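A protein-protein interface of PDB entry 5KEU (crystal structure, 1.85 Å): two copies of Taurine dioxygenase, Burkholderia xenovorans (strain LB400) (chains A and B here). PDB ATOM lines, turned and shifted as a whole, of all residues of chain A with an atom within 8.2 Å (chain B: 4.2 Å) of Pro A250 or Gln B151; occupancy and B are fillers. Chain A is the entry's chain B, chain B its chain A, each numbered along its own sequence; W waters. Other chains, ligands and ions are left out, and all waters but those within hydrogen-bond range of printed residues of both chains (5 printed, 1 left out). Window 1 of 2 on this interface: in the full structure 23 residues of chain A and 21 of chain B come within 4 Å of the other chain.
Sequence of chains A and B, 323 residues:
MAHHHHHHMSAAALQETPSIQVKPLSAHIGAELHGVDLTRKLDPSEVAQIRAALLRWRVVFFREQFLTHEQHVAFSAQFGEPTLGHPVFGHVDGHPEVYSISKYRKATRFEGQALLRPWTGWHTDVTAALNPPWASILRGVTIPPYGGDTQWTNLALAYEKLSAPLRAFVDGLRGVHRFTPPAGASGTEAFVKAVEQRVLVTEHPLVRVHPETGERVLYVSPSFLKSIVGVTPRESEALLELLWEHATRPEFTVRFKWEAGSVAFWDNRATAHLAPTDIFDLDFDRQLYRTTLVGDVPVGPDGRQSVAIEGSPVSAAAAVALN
Printed residues of chain B within 4 Å of Pro A250: Gln B151.
Of chain A, only Pro A250 (3.9 Å) comes within 4 Å of Gln B151.
Printed residues of chain A within 4 Å of Thr B253: Arg A255.
Of the printed residues of chain A, Arg B255 touches Ser A26, Thr A253 and Val A254.
Of the printed residues of chain B, Ser A26 touches Arg B255.
Of the printed residues of chain A, Val B254 touches Arg A255.
Of the printed residues of chain B, Arg A255 touches Thr B253 and Val B254.
His B273 touches none of the printed residues of chain A.
The nearest printed residue of chain B that does not touch Pro A250 is Leu B274 (4.01 Å).
Printed residues of chain B that touch a printed residue of chain A: Gln B151, Thr B253, Val B254 and Arg B255.
Among the printed residues, 6 pairs touch across the chains.
Among the printed residues, no Asp or Glu carboxylate lies within 4 Å of a Lys or Arg side-chain nitrogen of the other chain.
The backbone carbonyl oxygen (O) of Thr A253 lies within hydrogen-bond range of the guanidinium group (NH1) of Arg B255 (3.1 Å).
The backbone carbonyl oxygen (O) of Thr B253 lies within hydrogen-bond range of the guanidinium group (NH1) of Arg A255 (3.1 Å).
Water W3 bridges OE1 of Gln A151 (2.7 Å) and NH1 of Arg B255 (3.0 Å).
Water W4 lies within hydrogen-bond range of O of Thr B253 (2.7 Å) and NH2 of Arg A255 (2.9 Å).
Water W2 lies within hydrogen-bond range of the side-chain amide oxygen (OE1) of Gln B151 and the guanidinium group (NH1) of Arg A255.
Water W1 bridges the backbone carbonyl oxygen of Arg B255 (2.9 Å) and the guanidinium group of Arg A255 (3.3 Å).
Water W5 lies within hydrogen-bond range of the backbone NH of Arg A255 (2.9 Å) and the guanidinium group of Arg B255 (3.3 Å).
O of Pro A250 sits at hydrogen-bond distance from OG1 of Thr A253 (2.7 Å).
The backbone NH (N) of Leu B274 is in hydrogen-bond range of the backbone carbonyl oxygen (O) of Gln B151, 2.8 Å away.
The backbone carbonyl oxygen (O) of Val A254 lies within hydrogen-bond range of the backbone NH (N) of Trp A152 (3.0 Å).
The backbone carbonyl oxygen (O) of Trp B152 lies within hydrogen-bond range of the backbone NH (N) of Val B254, 2.9 Å away.
The backbone carbonyl oxygen of Ile A29 lies within hydrogen-bond range of the side-chain hydroxyl of Ser A26 (2.6 Å).
Thr A253 touches Arg B255, and with the chains exchanged Arg A255 touches Thr B253.
Val A254 touches Arg B255, and with the chains exchanged Arg A255 touches Val B254.
Positions printed for both chains: 122, 151, 152, 253, 254 and 255.
Among the printed residues, merely in contact across the chains: Ser A26 with Arg B255, Arg A255 with Val B254, Val A254 with Arg B255 and Pro A250 with Gln B151.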
ATOM      1  N   SER A  26       3.159  13.304 -25.495  1.00  0.00           N
ATOM      2  CA  SER A  26       2.817  14.449 -24.655  1.00  0.00           C
ATOM      3  C   SER A  26       3.401  14.164 -23.281  1.00  0.00           C
ATOM      4  O   SER A  26       4.004  13.116 -23.062  1.00  0.00           O
ATOM      5  CB  SER A  26       1.306  14.685 -24.588  1.00  0.00           C
ATOM      6  OG  SER A  26       0.673  13.723 -23.751  1.00  0.00           O
ATOM      7  N   ILE A  29       0.459  11.380 -21.763  1.00  0.00           N
ATOM      8  CA  ILE A  29      -0.371  10.391 -22.445  1.00  0.00           C
ATOM      9  C   ILE A  29       0.061  10.267 -23.897  1.00  0.00           C
ATOM     10  O   ILE A  29       0.318  11.263 -24.581  1.00  0.00           O
ATOM     11  CB  ILE A  29      -1.882  10.723 -22.318  1.00  0.00           C
ATOM     12  CG1 ILE A  29      -2.701   9.676 -23.069  1.00  0.00           C
ATOM     13  CG2 ILE A  29      -2.206  12.161 -22.826  1.00  0.00           C
ATOM     14  CD1 ILE A  29      -4.233   9.682 -22.740  1.00  0.00           C
ATOM     15  N   TRP A 122     -16.898  12.896 -25.430  1.00  0.00           N
ATOM     16  CA  TRP A 122     -15.859  12.198 -24.674  1.00  0.00           C
ATOM     17  C   TRP A 122     -16.459  11.021 -23.929  1.00  0.00           C
ATOM     18  O   TRP A 122     -17.491  11.167 -23.268  1.00  0.00           O
ATOM     19  CB  TRP A 122     -15.196  13.144 -23.679  1.00  0.00           C
ATOM     20  CG  TRP A 122     -14.235  14.092 -24.310  1.00  0.00           C
ATOM     21  CD1 TRP A 122     -14.490  15.374 -24.756  1.00  0.00           C
ATOM     22  CD2 TRP A 122     -12.852  13.840 -24.573  1.00  0.00           C
ATOM     23  NE1 TRP A 122     -13.334  15.926 -25.269  1.00  0.00           N
ATOM     24  CE2 TRP A 122     -12.317  15.007 -25.170  1.00  0.00           C
ATOM     25  CE3 TRP A 122     -12.013  12.734 -24.377  1.00  0.00           C
ATOM     26  CZ2 TRP A 122     -10.980  15.104 -25.543  1.00  0.00           C
ATOM     27  CZ3 TRP A 122     -10.669  12.833 -24.746  1.00  0.00           C
ATOM     28  CH2 TRP A 122     -10.174  14.008 -25.331  1.00  0.00           C
ATOM     29  N   GLN A 151      -8.886  11.810 -30.214  1.00  0.00           N
ATOM     30  CA  GLN A 151      -8.208  12.298 -29.017  1.00  0.00           C
ATOM     31  C   GLN A 151      -8.476  11.370 -27.836  1.00  0.00           C
ATOM     32  O   GLN A 151      -9.541  10.755 -27.744  1.00  0.00           O
ATOM     33  CB  GLN A 151      -8.651  13.699 -28.637  1.00  0.00           C
ATOM     34  CG  GLN A 151      -8.502  14.716 -29.778  1.00  0.00           C
ATOM     35  CD  GLN A 151      -8.537  16.143 -29.288  1.00  0.00           C
ATOM     36  OE1 GLN A 151      -7.848  16.494 -28.333  1.00  0.00           O
ATOM     37  NE2 GLN A 151      -9.319  16.987 -29.964  1.00  0.00           N
ATOM     38  N   TRP A 152      -7.513  11.317 -26.911  1.00  0.00           N
ATOM     39  CA  TRP A 152      -7.645  10.559 -25.668  1.00  0.00           C
ATOM     40  C   TRP A 152      -7.313  11.477 -24.507  1.00  0.00           C
ATOM     41  O   TRP A 152      -6.476  12.376 -24.641  1.00  0.00           O
ATOM     42  CB  TRP A 152      -6.681   9.341 -25.604  1.00  0.00           C
ATOM     43  CG  TRP A 152      -7.096   8.197 -26.494  1.00  0.00           C
ATOM     44  CD1 TRP A 152      -7.732   7.045 -26.109  1.00  0.00           C
ATOM     45  CD2 TRP A 152      -6.901   8.096 -27.913  1.00  0.00           C
ATOM     46  NE1 TRP A 152      -7.956   6.233 -27.210  1.00  0.00           N
ATOM     47  CE2 TRP A 152      -7.454   6.853 -28.325  1.00  0.00           C
ATOM     48  CE3 TRP A 152      -6.316   8.923 -28.871  1.00  0.00           C
ATOM     49  CZ2 TRP A 152      -7.431   6.426 -29.655  1.00  0.00           C
ATOM     50  CZ3 TRP A 152      -6.298   8.490 -30.206  1.00  0.00           C
ATOM     51  CH2 TRP A 152      -6.834   7.251 -30.575  1.00  0.00           C
ATOM     52  N   THR A 153      -7.918  11.215 -23.347  1.00  0.00           N
ATOM     53  CA  THR A 153      -7.527  11.937 -22.148  1.00  0.00           C
ATOM     54  C   THR A 153      -7.154  10.943 -21.049  1.00  0.00           C
ATOM     55  O   THR A 153      -7.666   9.818 -20.995  1.00  0.00           O
ATOM     56  CB  THR A 153      -8.632  12.888 -21.689  1.00  0.00           C
ATOM     57  OG1 THR A 153      -8.145  13.690 -20.606  1.00  0.00           O
ATOM     58  CG2 THR A 153      -9.899  12.110 -21.251  1.00  0.00           C
ATOM     59  N   ASN A 154      -6.248  11.378 -20.182  1.00  0.00           N
ATOM     60  CA  ASN A 154      -5.667  10.547 -19.130  1.00  0.00           C
ATOM     61  C   ASN A 154      -6.475  10.756 -17.853  1.00  0.00           C
ATOM     62  O   ASN A 154      -6.338  11.777 -17.178  1.00  0.00           O
ATOM     63  CB  ASN A 154      -4.195  10.912 -18.936  1.00  0.00           C
ATOM     64  CG  ASN A 154      -3.508  10.048 -17.893  1.00  0.00           C
ATOM     65  OD1 ASN A 154      -4.155   9.463 -17.033  1.00  0.00           O
ATOM     66  ND2 ASN A 154      -2.185   9.990 -17.953  1.00  0.00           N
ATOM     67  N   LEU A 157      -4.377  10.718 -14.444  1.00  0.00           N
ATOM     68  CA  LEU A 157      -3.883  12.067 -14.200  1.00  0.00           C
ATOM     69  C   LEU A 157      -5.007  13.004 -13.771  1.00  0.00           C
ATOM     70  O   LEU A 157      -4.831  13.828 -12.860  1.00  0.00           O
ATOM     71  CB  LEU A 157      -3.209  12.596 -15.474  1.00  0.00           C
ATOM     72  CG  LEU A 157      -2.637  13.998 -15.404  1.00  0.00           C
ATOM     73  CD1 LEU A 157      -1.531  14.040 -14.353  1.00  0.00           C
ATOM     74  CD2 LEU A 157      -2.126  14.373 -16.783  1.00  0.00           C
ATOM     75  N   GLU A 245     -15.535  18.978 -17.152  1.00  0.00           N
ATOM     76  CA  GLU A 245     -14.656  20.065 -17.573  1.00  0.00           C
ATOM     77  C   GLU A 245     -13.214  19.760 -17.180  1.00  0.00           C
ATOM     78  O   GLU A 245     -12.279  19.930 -17.971  1.00  0.00           O
ATOM     79  CB  GLU A 245     -15.190  21.360 -16.942  1.00  0.00           C
ATOM     80  CG  GLU A 245     -14.333  22.596 -16.877  1.00  0.00           C
ATOM     81  CD  GLU A 245     -15.034  23.736 -16.098  1.00  0.00           C
ATOM     82  OE1 GLU A 245     -15.219  23.637 -14.838  1.00  0.00           O
ATOM     83  OE2 GLU A 245     -15.433  24.722 -16.766  1.00  0.00           O
ATOM     84  N   HIS A 246     -13.029  19.278 -15.952  1.00  0.00           N
ATOM     85  CA  HIS A 246     -11.693  18.955 -15.469  1.00  0.00           C
ATOM     86  C   HIS A 246     -11.072  17.812 -16.274  1.00  0.00           C
ATOM     87  O   HIS A 246      -9.901  17.869 -16.659  1.00  0.00           O
ATOM     88  CB  HIS A 246     -11.778  18.591 -13.979  1.00  0.00           C
ATOM     89  CG  HIS A 246     -10.471  18.136 -13.400  1.00  0.00           C
ATOM     90  ND1 HIS A 246      -9.434  19.006 -13.135  1.00  0.00           N
ATOM     91  CD2 HIS A 246     -10.022  16.901 -13.075  1.00  0.00           C
ATOM     92  CE1 HIS A 246      -8.406  18.326 -12.650  1.00  0.00           C
ATOM     93  NE2 HIS A 246      -8.733  17.046 -12.613  1.00  0.00           N
ATOM     94  N   ALA A 247     -11.840  16.760 -16.540  1.00  0.00           N
ATOM     95  CA  ALA A 247     -11.263  15.572 -17.155  1.00  0.00           C
ATOM     96  C   ALA A 247     -10.834  15.813 -18.594  1.00  0.00           C
ATOM     97  O   ALA A 247     -10.106  14.985 -19.147  1.00  0.00           O
ATOM     98  CB  ALA A 247     -12.262  14.403 -17.120  1.00  0.00           C
ATOM     99  N   THR A 248     -11.295  16.899 -19.215  1.00  0.00           N
ATOM    100  CA  THR A 248     -10.982  17.183 -20.602  1.00  0.00           C
ATOM    101  C   THR A 248     -10.040  18.377 -20.739  1.00  0.00           C
ATOM    102  O   THR A 248      -9.969  18.973 -21.816  1.00  0.00           O
ATOM    103  CB  THR A 248     -12.268  17.397 -21.413  1.00  0.00           C
ATOM    104  OG1 THR A 248     -13.055  18.438 -20.824  1.00  0.00           O
ATOM    105  CG2 THR A 248     -13.094  16.103 -21.434  1.00  0.00           C
ATOM    106  N   ARG A 249      -9.326  18.740 -19.667  1.00  0.00           N
ATOM    107  CA  ARG A 249      -8.267  19.742 -19.785  1.00  0.00           C
ATOM    108  C   ARG A 249      -7.333  19.364 -20.936  1.00  0.00           C
ATOM    109  O   ARG A 249      -6.902  18.206 -21.026  1.00  0.00           O
ATOM    110  CB  ARG A 249      -7.425  19.840 -18.496  1.00  0.00           C
ATOM    111  CG  ARG A 249      -8.086  20.454 -17.256  1.00  0.00           C
ATOM    112  CD  ARG A 249      -8.418  21.932 -17.428  1.00  0.00           C
ATOM    113  NE  ARG A 249      -7.288  22.628 -18.024  1.00  0.00           N
ATOM    114  CZ  ARG A 249      -7.392  23.699 -18.796  1.00  0.00           C
ATOM    115  NH1 ARG A 249      -6.294  24.236 -19.320  1.00  0.00           N
ATOM    116  NH2 ARG A 249      -8.590  24.233 -19.034  1.00  0.00           N
ATOM    117  N   PRO A 250      -6.940  20.321 -21.779  1.00  0.00           N
ATOM    118  CA  PRO A 250      -6.065  19.985 -22.918  1.00  0.00           C
ATOM    119  C   PRO A 250      -4.765  19.333 -22.499  1.00  0.00           C
ATOM    120  O   PRO A 250      -4.255  18.453 -23.205  1.00  0.00           O
ATOM    121  CB  PRO A 250      -5.796  21.348 -23.578  1.00  0.00           C
ATOM    122  CG  PRO A 250      -6.693  22.321 -22.942  1.00  0.00           C
ATOM    123  CD  PRO A 250      -7.250  21.753 -21.676  1.00  0.00           C
ATOM    124  N   GLU A 251      -4.205  19.751 -21.360  1.00  0.00           N
ATOM    125  CA  GLU A 251      -2.936  19.177 -20.916  1.00  0.00           C
ATOM    126  C   GLU A 251      -3.062  17.724 -20.467  1.00  0.00           C
ATOM    127  O   GLU A 251      -2.033  17.078 -20.251  1.00  0.00           O
ATOM    128  CB  GLU A 251      -2.325  20.052 -19.794  1.00  0.00           C
ATOM    129  CG  GLU A 251      -3.194  20.195 -18.525  1.00  0.00           C
ATOM    130  CD  GLU A 251      -4.135  21.402 -18.559  1.00  0.00           C
ATOM    131  OE1 GLU A 251      -4.560  21.845 -17.469  1.00  0.00           O
ATOM    132  OE2 GLU A 251      -4.449  21.921 -19.664  1.00  0.00           O
ATOM    133  N   PHE A 252      -4.277  17.174 -20.357  1.00  0.00           N
ATOM    134  CA  PHE A 252      -4.446  15.752 -20.068  1.00  0.00           C
ATOM    135  C   PHE A 252      -4.615  14.914 -21.336  1.00  0.00           C
ATOM    136  O   PHE A 252      -4.808  13.700 -21.229  1.00  0.00           O
ATOM    137  CB  PHE A 252      -5.673  15.486 -19.165  1.00  0.00           C
ATOM    138  CG  PHE A 252      -5.699  16.264 -17.863  1.00  0.00           C
ATOM    139  CD1 PHE A 252      -4.547  16.813 -17.324  1.00  0.00           C
ATOM    140  CD2 PHE A 252      -6.893  16.407 -17.166  1.00  0.00           C
ATOM    141  CE1 PHE A 252      -4.589  17.535 -16.116  1.00  0.00           C
ATOM    142  CE2 PHE A 252      -6.946  17.115 -15.959  1.00  0.00           C
ATOM    143  CZ  PHE A 252      -5.781  17.677 -15.432  1.00  0.00           C
ATOM    144  N   THR A 253      -4.528  15.518 -22.520  1.00  0.00           N
ATOM    145  CA  THR A 253      -4.953  14.869 -23.753  1.00  0.00           C
ATOM    146  C   THR A 253      -3.814  14.663 -24.742  1.00  0.00           C
ATOM    147  O   THR A 253      -2.762  15.303 -24.681  1.00  0.00           O
ATOM    148  CB  THR A 253      -6.056  15.684 -24.464  1.00  0.00           C
ATOM    149  OG1 THR A 253      -5.499  16.908 -24.987  1.00  0.00           O
ATOM    150  CG2 THR A 253      -7.180  16.002 -23.493  1.00  0.00           C
ATOM    151  N   VAL A 254      -4.063  13.756 -25.685  1.00  0.00           N
ATOM    152  CA  VAL A 254      -3.215  13.582 -26.856  1.00  0.00           C
ATOM    153  C   VAL A 254      -4.134  13.447 -28.063  1.00  0.00           C
ATOM    154  O   VAL A 254      -5.240  12.901 -27.964  1.00  0.00           O
ATOM    155  CB  VAL A 254      -2.282  12.352 -26.729  1.00  0.00           C
ATOM    156  CG1 VAL A 254      -3.088  11.045 -26.749  1.00  0.00           C
ATOM    157  CG2 VAL A 254      -1.238  12.345 -27.854  1.00  0.00           C
ATOM    158  N   ARG A 255      -3.679  13.962 -29.203  1.00  0.00           N
ATOM    159  CA  ARG A 255      -4.432  13.903 -30.450  1.00  0.00           C
ATOM    160  C   ARG A 255      -3.650  13.095 -31.482  1.00  0.00           C
ATOM    161  O   ARG A 255      -2.422  13.195 -31.556  1.00  0.00           O
ATOM    162  CB  ARG A 255      -4.705  15.336 -30.962  1.00  0.00           C
ATOM    163  CG  ARG A 255      -5.463  15.404 -32.291  1.00  0.00           C
ATOM    164  CD  ARG A 255      -5.920  16.833 -32.538  1.00  0.00           C
ATOM    165  NE  ARG A 255      -6.546  17.019 -33.845  1.00  0.00           N
ATOM    166  CZ  ARG A 255      -7.193  18.119 -34.204  1.00  0.00           C
ATOM    167  NH1 ARG A 255      -7.326  19.115 -33.337  1.00  0.00           N
ATOM    168  NH2 ARG A 255      -7.717  18.216 -35.426  1.00  0.00           N
ATOM    169  N   TRP B 122      -6.457  30.587 -24.085  1.00  0.00           N
ATOM    170  CA  TRP B 122      -6.686  30.858 -25.495  1.00  0.00           C
ATOM    171  C   TRP B 122      -6.682  32.359 -25.734  1.00  0.00           C
ATOM    172  O   TRP B 122      -7.338  33.106 -24.998  1.00  0.00           O
ATOM    173  CB  TRP B 122      -8.028  30.267 -25.930  1.00  0.00           C
ATOM    174  CG  TRP B 122      -8.013  28.768 -26.133  1.00  0.00           C
ATOM    175  CD1 TRP B 122      -8.356  27.797 -25.223  1.00  0.00           C
ATOM    176  CD2 TRP B 122      -7.655  28.088 -27.333  1.00  0.00           C
ATOM    177  NE1 TRP B 122      -8.217  26.548 -25.797  1.00  0.00           N
ATOM    178  CE2 TRP B 122      -7.800  26.701 -27.095  1.00  0.00           C
ATOM    179  CE3 TRP B 122      -7.203  28.514 -28.584  1.00  0.00           C
ATOM    180  CZ2 TRP B 122      -7.524  25.740 -28.075  1.00  0.00           C
ATOM    181  CZ3 TRP B 122      -6.929  27.556 -29.563  1.00  0.00           C
ATOM    182  CH2 TRP B 122      -7.094  26.188 -29.305  1.00  0.00           C
ATOM    183  N   THR B 150       1.470  23.277 -29.292  1.00  0.00           N
ATOM    184  CA  THR B 150       0.651  24.474 -29.402  1.00  0.00           C
ATOM    185  C   THR B 150      -0.626  24.155 -30.169  1.00  0.00           C
ATOM    186  O   THR B 150      -0.630  23.289 -31.048  1.00  0.00           O
ATOM    187  CB  THR B 150       1.438  25.583 -30.115  1.00  0.00           C
ATOM    188  OG1 THR B 150       2.689  25.755 -29.432  1.00  0.00           O
ATOM    189  CG2 THR B 150       0.662  26.900 -30.126  1.00  0.00           C
ATOM    190  N   GLN B 151      -1.721  24.848 -29.827  1.00  0.00           N
ATOM    191  CA  GLN B 151      -2.972  24.693 -30.559  1.00  0.00           C
ATOM    192  C   GLN B 151      -3.461  26.027 -31.102  1.00  0.00           C
ATOM    193  O   GLN B 151      -3.210  27.085 -30.519  1.00  0.00           O
ATOM    194  CB  GLN B 151      -4.065  24.095 -29.692  1.00  0.00           C
ATOM    195  CG  GLN B 151      -3.610  22.816 -28.980  1.00  0.00           C
ATOM    196  CD  GLN B 151      -4.788  21.996 -28.514  1.00  0.00           C
ATOM    197  OE1 GLN B 151      -5.777  21.861 -29.226  1.00  0.00           O
ATOM    198  NE2 GLN B 151      -4.684  21.427 -27.321  1.00  0.00           N
ATOM    199  N   TRP B 152      -4.201  25.953 -32.207  1.00  0.00           N
ATOM    200  CA  TRP B 152      -4.859  27.104 -32.806  1.00  0.00           C
ATOM    201  C   TRP B 152      -6.326  26.772 -33.046  1.00  0.00           C
ATOM    202  O   TRP B 152      -6.675  25.617 -33.295  1.00  0.00           O
ATOM    203  CB  TRP B 152      -4.245  27.495 -34.153  1.00  0.00           C
ATOM    204  CG  TRP B 152      -2.882  28.126 -34.066  1.00  0.00           C
ATOM    205  CD1 TRP B 152      -2.597  29.459 -34.185  1.00  0.00           C
ATOM    206  CD2 TRP B 152      -1.623  27.461 -33.862  1.00  0.00           C
ATOM    207  NE1 TRP B 152      -1.236  29.665 -34.073  1.00  0.00           N
ATOM    208  CE2 TRP B 152      -0.618  28.461 -33.863  1.00  0.00           C
ATOM    209  CE3 TRP B 152      -1.248  26.125 -33.669  1.00  0.00           C
ATOM    210  CZ2 TRP B 152       0.738  28.170 -33.695  1.00  0.00           C
ATOM    211  CZ3 TRP B 152       0.117  25.831 -33.501  1.00  0.00           C
ATOM    212  CH2 TRP B 152       1.084  26.852 -33.508  1.00  0.00           C
ATOM    213  N   THR B 253     -10.157  23.277 -34.171  1.00  0.00           N
ATOM    214  CA  THR B 253      -8.774  23.434 -33.739  1.00  0.00           C
ATOM    215  C   THR B 253      -7.817  22.529 -34.501  1.00  0.00           C
ATOM    216  O   THR B 253      -8.206  21.527 -35.114  1.00  0.00           O
ATOM    217  CB  THR B 253      -8.614  23.138 -32.243  1.00  0.00           C
ATOM    218  OG1 THR B 253      -8.848  21.744 -32.010  1.00  0.00           O
ATOM    219  CG2 THR B 253      -9.593  23.961 -31.436  1.00  0.00           C
ATOM    220  N   VAL B 254      -6.537  22.885 -34.399  1.00  0.00           N
ATOM    221  CA  VAL B 254      -5.433  22.043 -34.841  1.00  0.00           C
ATOM    222  C   VAL B 254      -4.367  22.099 -33.764  1.00  0.00           C
ATOM    223  O   VAL B 254      -4.176  23.137 -33.121  1.00  0.00           O
ATOM    224  CB  VAL B 254      -4.860  22.485 -36.208  1.00  0.00           C
ATOM    225  CG1 VAL B 254      -4.184  23.870 -36.121  1.00  0.00           C
ATOM    226  CG2 VAL B 254      -3.879  21.429 -36.761  1.00  0.00           C
ATOM    227  N   ARG B 255      -3.683  20.979 -33.562  1.00  0.00           N
ATOM    228  CA  ARG B 255      -2.601  20.872 -32.597  1.00  0.00           C
ATOM    229  C   ARG B 255      -1.301  20.581 -33.335  1.00  0.00           C
ATOM    230  O   ARG B 255      -1.295  19.834 -34.316  1.00  0.00           O
ATOM    231  CB  ARG B 255      -2.913  19.766 -31.588  1.00  0.00           C
ATOM    232  CG  ARG B 255      -1.842  19.516 -30.531  1.00  0.00           C
ATOM    233  CD  ARG B 255      -2.454  18.688 -29.380  1.00  0.00           C
ATOM    234  NE  ARG B 255      -1.448  18.247 -28.415  1.00  0.00           N
ATOM    235  CZ  ARG B 255      -1.733  17.622 -27.277  1.00  0.00           C
ATOM    236  NH1 ARG B 255      -3.007  17.403 -26.949  1.00  0.00           N
ATOM    237  NH2 ARG B 255      -0.751  17.243 -26.459  1.00  0.00           N
ATOM    238  N   HIS B 273      -4.870  31.192 -30.237  1.00  0.00           N
ATOM    239  CA  HIS B 273      -3.986  30.054 -30.006  1.00  0.00           C
ATOM    240  C   HIS B 273      -3.805  29.806 -28.515  1.00  0.00           C
ATOM    241  O   HIS B 273      -4.167  30.626 -27.665  1.00  0.00           O
ATOM    242  CB  HIS B 273      -2.616  30.220 -30.696  1.00  0.00           C
ATOM    243  CG  HIS B 273      -1.886  31.482 -30.336  1.00  0.00           C
ATOM    244  ND1 HIS B 273      -2.171  32.697 -30.923  1.00  0.00           N
ATOM    245  CD2 HIS B 273      -0.864  31.712 -29.474  1.00  0.00           C
ATOM    246  CE1 HIS B 273      -1.373  33.625 -30.425  1.00  0.00           C
ATOM    247  NE2 HIS B 273      -0.570  33.059 -29.544  1.00  0.00           N
ATOM    248  N   LEU B 274      -3.221  28.646 -28.217  1.00  0.00           N
ATOM    249  CA  LEU B 274      -3.104  28.137 -26.857  1.00  0.00           C
ATOM    250  C   LEU B 274      -1.679  27.649 -26.621  1.00  0.00           C
ATOM    251  O   LEU B 274      -1.277  26.626 -27.177  1.00  0.00           O
ATOM    252  CB  LEU B 274      -4.102  26.996 -26.633  1.00  0.00           C
ATOM    253  CG  LEU B 274      -4.021  26.333 -25.263  1.00  0.00           C
ATOM    254  CD1 LEU B 274      -4.457  27.295 -24.163  1.00  0.00           C
ATOM    255  CD2 LEU B 274      -4.889  25.052 -25.253  1.00  0.00           C
HETATM  256  O   HOH W   1      -3.690  18.366 -34.841  1.00  0.00           O
HETATM  257  O   HOH W   2      -6.475  19.545 -30.631  1.00  0.00           O
HETATM  258  O   HOH W   3      -5.577  17.910 -28.439  1.00  0.00           O
HETATM  259  O   HOH W   4     -10.070  19.795 -35.994  1.00  0.00           O
HETATM  260  O   HOH W   5      -1.200  15.282 -29.928  1.00  0.00           O
